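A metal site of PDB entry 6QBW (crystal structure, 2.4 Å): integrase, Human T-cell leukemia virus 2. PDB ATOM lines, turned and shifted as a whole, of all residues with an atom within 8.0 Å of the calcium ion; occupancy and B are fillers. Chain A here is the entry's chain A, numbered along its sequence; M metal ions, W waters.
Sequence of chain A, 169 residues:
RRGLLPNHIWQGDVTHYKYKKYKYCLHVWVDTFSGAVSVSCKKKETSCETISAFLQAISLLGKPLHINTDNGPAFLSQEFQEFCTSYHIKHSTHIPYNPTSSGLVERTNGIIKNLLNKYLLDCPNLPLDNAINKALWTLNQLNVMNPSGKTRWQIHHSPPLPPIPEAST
Within 4 Å of the calcium ion: Asp 13, Val 14 and Asp 70. The nearest printed residue that does not touch the calcium ion is Thr 15 (4.9 Å).
The side-chain carboxylate (OD1) of Asp 70 lies within hydrogen-bond range of the backbone NH (N) of Gly 72, at 3.0 Å. The side-chain carboxylate (OD2) of Asp 13 sits at hydrogen-bond distance from the side-chain amide nitrogen (ND2) of Asn 109 (2.9 Å).
Water W1 lies within hydrogen-bond range of OD1 of Asp 70 (2.7 Å) and N of Val 14 (3.3 Å).
The calcium ion is bound by water W3 (2.3 Å), water W1 (2.4 Å), water W2 (2.5 Å), the side-chain carboxylate (OD2) of Asp 70 (2.6 Å), the side-chain carboxylate (OD1) of Asp 13 (2.6 Å) and the backbone carbonyl oxygen (O) of Val 14 (2.8 Å). The calcium ion has six donor atoms within binding distance.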
ATOM      1  N   GLY A  12     -20.602 -12.148  10.187  1.00  0.00           N
ATOM      2  CA  GLY A  12     -22.013 -11.856   9.969  1.00  0.00           C
ATOM      3  C   GLY A  12     -22.361 -11.827   8.497  1.00  0.00           C
ATOM      4  O   GLY A  12     -21.558 -11.384   7.680  1.00  0.00           O
ATOM      5  N   ASP A  13     -23.556 -12.308   8.172  1.00  0.00           N
ATOM      6  CA  ASP A  13     -24.040 -12.300   6.796  1.00  0.00           C
ATOM      7  C   ASP A  13     -25.562 -12.140   6.762  1.00  0.00           C
ATOM      8  O   ASP A  13     -26.252 -12.508   7.710  1.00  0.00           O
ATOM      9  CB  ASP A  13     -23.634 -13.592   6.096  1.00  0.00           C
ATOM     10  CG  ASP A  13     -23.962 -13.582   4.604  1.00  0.00           C
ATOM     11  OD1 ASP A  13     -23.819 -12.533   3.933  1.00  0.00           O
ATOM     12  OD2 ASP A  13     -24.352 -14.654   4.091  1.00  0.00           O
ATOM     13  N   VAL A  14     -26.067 -11.568   5.681  1.00  0.00           N
ATOM     14  CA  VAL A  14     -27.487 -11.640   5.387  1.00  0.00           C
ATOM     15  C   VAL A  14     -27.662 -12.476   4.125  1.00  0.00           C
ATOM     16  O   VAL A  14     -27.101 -12.171   3.069  1.00  0.00           O
ATOM     17  CB  VAL A  14     -28.124 -10.250   5.205  1.00  0.00           C
ATOM     18  CG1 VAL A  14     -29.622 -10.393   4.945  1.00  0.00           C
ATOM     19  CG2 VAL A  14     -27.863  -9.384   6.424  1.00  0.00           C
ATOM     20  N   THR A  15     -28.418 -13.557   4.253  1.00  0.00           N
ATOM     21  CA  THR A  15     -28.681 -14.470   3.149  1.00  0.00           C
ATOM     22  C   THR A  15     -30.176 -14.631   2.982  1.00  0.00           C
ATOM     23  O   THR A  15     -30.937 -14.466   3.933  1.00  0.00           O
ATOM     24  CB  THR A  15     -27.996 -15.846   3.358  1.00  0.00           C
ATOM     25  OG1 THR A  15     -28.291 -16.697   2.241  1.00  0.00           O
ATOM     26  CG2 THR A  15     -28.481 -16.537   4.631  1.00  0.00           C
ATOM     27  N   HIS A  16     -30.592 -14.941   1.757  1.00  0.00           N
ATOM     28  CA  HIS A  16     -32.005 -15.131   1.460  1.00  0.00           C
ATOM     29  C   HIS A  16     -32.418 -16.571   1.716  1.00  0.00           C
ATOM     30  O   HIS A  16     -31.635 -17.495   1.532  1.00  0.00           O
ATOM     31  CB  HIS A  16     -32.289 -14.735   0.005  1.00  0.00           C
ATOM     32  CG  HIS A  16     -32.048 -13.282  -0.267  1.00  0.00           C
ATOM     33  ND1 HIS A  16     -32.992 -12.307  -0.007  1.00  0.00           N
ATOM     34  CD2 HIS A  16     -30.966 -12.631  -0.749  1.00  0.00           C
ATOM     35  CE1 HIS A  16     -32.504 -11.121  -0.333  1.00  0.00           C
ATOM     36  NE2 HIS A  16     -31.275 -11.293  -0.777  1.00  0.00           N
ATOM     37  N   LEU A  26     -32.315 -13.830   6.136  1.00  0.00           N
ATOM     38  CA  LEU A  26     -31.704 -14.441   7.301  1.00  0.00           C
ATOM     39  C   LEU A  26     -30.460 -13.667   7.673  1.00  0.00           C
ATOM     40  O   LEU A  26     -29.459 -13.744   6.980  1.00  0.00           O
ATOM     41  CB  LEU A  26     -31.344 -15.905   7.034  1.00  0.00           C
ATOM     42  CG  LEU A  26     -32.493 -16.887   6.821  1.00  0.00           C
ATOM     43  CD1 LEU A  26     -31.944 -18.307   6.883  1.00  0.00           C
ATOM     44  CD2 LEU A  26     -33.607 -16.695   7.840  1.00  0.00           C
ATOM     45  N   GLU A  45     -34.188  -5.724   4.986  1.00  0.00           N
ATOM     46  CA  GLU A  45     -32.750  -5.723   5.279  1.00  0.00           C
ATOM     47  C   GLU A  45     -32.229  -4.327   5.655  1.00  0.00           C
ATOM     48  O   GLU A  45     -31.011  -4.095   5.670  1.00  0.00           O
ATOM     49  CB  GLU A  45     -32.006  -6.244   4.045  1.00  0.00           C
ATOM     50  CG  GLU A  45     -30.610  -6.771   4.296  1.00  0.00           C
ATOM     51  CD  GLU A  45     -29.848  -7.017   3.004  1.00  0.00           C
ATOM     52  OE1 GLU A  45     -30.317  -7.831   2.168  1.00  0.00           O
ATOM     53  OE2 GLU A  45     -28.772  -6.407   2.822  1.00  0.00           O
ATOM     54  N   THR A  69     -17.926  -8.791   7.906  1.00  0.00           N
ATOM     55  CA  THR A  69     -19.073  -8.981   7.018  1.00  0.00           C
ATOM     56  C   THR A  69     -18.664  -8.780   5.568  1.00  0.00           C
ATOM     57  O   THR A  69     -17.533  -8.411   5.272  1.00  0.00           O
ATOM     58  CB  THR A  69     -20.212  -8.000   7.348  1.00  0.00           C
ATOM     59  OG1 THR A  69     -19.833  -6.668   6.975  1.00  0.00           O
ATOM     60  CG2 THR A  69     -20.559  -8.049   8.838  1.00  0.00           C
ATOM     61  N   ASP A  70     -19.614  -9.037   4.665  1.00  0.00           N
ATOM     62  CA  ASP A  70     -19.430  -8.706   3.258  1.00  0.00           C
ATOM     63  C   ASP A  70     -19.807  -7.236   3.036  1.00  0.00           C
ATOM     64  O   ASP A  70     -20.125  -6.531   4.000  1.00  0.00           O
ATOM     65  CB  ASP A  70     -20.240  -9.678   2.356  1.00  0.00           C
ATOM     66  CG  ASP A  70     -21.735  -9.664   2.639  1.00  0.00           C
ATOM     67  OD1 ASP A  70     -22.252  -8.730   3.288  1.00  0.00           O
ATOM     68  OD2 ASP A  70     -22.428 -10.603   2.199  1.00  0.00           O
ATOM     69  N   ASN A  71     -19.782  -6.799   1.784  1.00  0.00           N
ATOM     70  CA  ASN A  71     -20.161  -5.422   1.422  1.00  0.00           C
ATOM     71  C   ASN A  71     -21.653  -5.287   1.137  1.00  0.00           C
ATOM     72  O   ASN A  71     -22.067  -4.379   0.416  1.00  0.00           O
ATOM     73  CB  ASN A  71     -19.382  -4.968   0.192  1.00  0.00           C
ATOM     74  CG  ASN A  71     -17.892  -4.927   0.446  1.00  0.00           C
ATOM     75  OD1 ASN A  71     -17.383  -5.632   1.311  1.00  0.00           O
ATOM     76  ND2 ASN A  71     -17.185  -4.090  -0.324  1.00  0.00           N
ATOM     77  N   GLY A  72     -22.474  -6.177   1.693  1.00  0.00           N
ATOM     78  CA  GLY A  72     -23.909  -6.095   1.501  1.00  0.00           C
ATOM     79  C   GLY A  72     -24.416  -4.736   1.929  1.00  0.00           C
ATOM     80  O   GLY A  72     -23.777  -4.054   2.748  1.00  0.00           O
ATOM     81  N   PRO A  73     -25.571  -4.313   1.382  1.00  0.00           N
ATOM     82  CA  PRO A  73     -26.092  -2.989   1.739  1.00  0.00           C
ATOM     83  C   PRO A  73     -26.413  -2.843   3.230  1.00  0.00           C
ATOM     84  O   PRO A  73     -26.364  -1.733   3.760  1.00  0.00           O
ATOM     85  CB  PRO A  73     -27.349  -2.852   0.872  1.00  0.00           C
ATOM     86  CG  PRO A  73     -27.733  -4.248   0.483  1.00  0.00           C
ATOM     87  CD  PRO A  73     -26.477  -5.064   0.491  1.00  0.00           C
ATOM     88  N   ALA A  74     -26.716  -3.962   3.890  1.00  0.00           N
ATOM     89  CA  ALA A  74     -26.965  -3.988   5.336  1.00  0.00           C
ATOM     90  C   ALA A  74     -25.774  -3.462   6.158  1.00  0.00           C
ATOM     91  O   ALA A  74     -25.951  -2.673   7.089  1.00  0.00           O
ATOM     92  CB  ALA A  74     -27.298  -5.405   5.782  1.00  0.00           C
ATOM     93  N   PHE A  75     -24.570  -3.895   5.792  1.00  0.00           N
ATOM     94  CA  PHE A  75     -23.368  -3.577   6.555  1.00  0.00           C
ATOM     95  C   PHE A  75     -22.571  -2.405   5.981  1.00  0.00           C
ATOM     96  O   PHE A  75     -21.432  -2.165   6.373  1.00  0.00           O
ATOM     97  CB  PHE A  75     -22.466  -4.811   6.647  1.00  0.00           C
ATOM     98  CG  PHE A  75     -23.190  -6.076   6.985  1.00  0.00           C
ATOM     99  CD1 PHE A  75     -23.879  -6.189   8.191  1.00  0.00           C
ATOM    100  CD2 PHE A  75     -23.205  -7.148   6.105  1.00  0.00           C
ATOM    101  CE1 PHE A  75     -24.559  -7.357   8.505  1.00  0.00           C
ATOM    102  CE2 PHE A  75     -23.876  -8.314   6.416  1.00  0.00           C
ATOM    103  CZ  PHE A  75     -24.557  -8.425   7.619  1.00  0.00           C
ATOM    104  N   ASN A 109     -24.587 -20.891   7.123  1.00  0.00           N
ATOM    105  CA  ASN A 109     -25.831 -20.670   6.386  1.00  0.00           C
ATOM    106  C   ASN A 109     -26.397 -21.981   5.817  1.00  0.00           C
ATOM    107  O   ASN A 109     -27.606 -22.219   5.889  1.00  0.00           O
ATOM    108  CB  ASN A 109     -25.597 -19.685   5.235  1.00  0.00           C
ATOM    109  CG  ASN A 109     -25.410 -18.259   5.705  1.00  0.00           C
ATOM    110  OD1 ASN A 109     -25.463 -17.977   6.906  1.00  0.00           O
ATOM    111  ND2 ASN A 109     -25.180 -17.362   4.761  1.00  0.00           N
HETATM  112 CA    CA M   1     -24.783 -11.506   1.726  1.00  0.00          CA
HETATM  113  O   HOH W   1     -24.819  -9.658   3.324  1.00  0.00           O
HETATM  114  O   HOH W   2     -23.768 -13.784   1.366  1.00  0.00           O
HETATM  115  O   HOH W   3     -26.691 -11.104   0.491  1.00  0.00           O
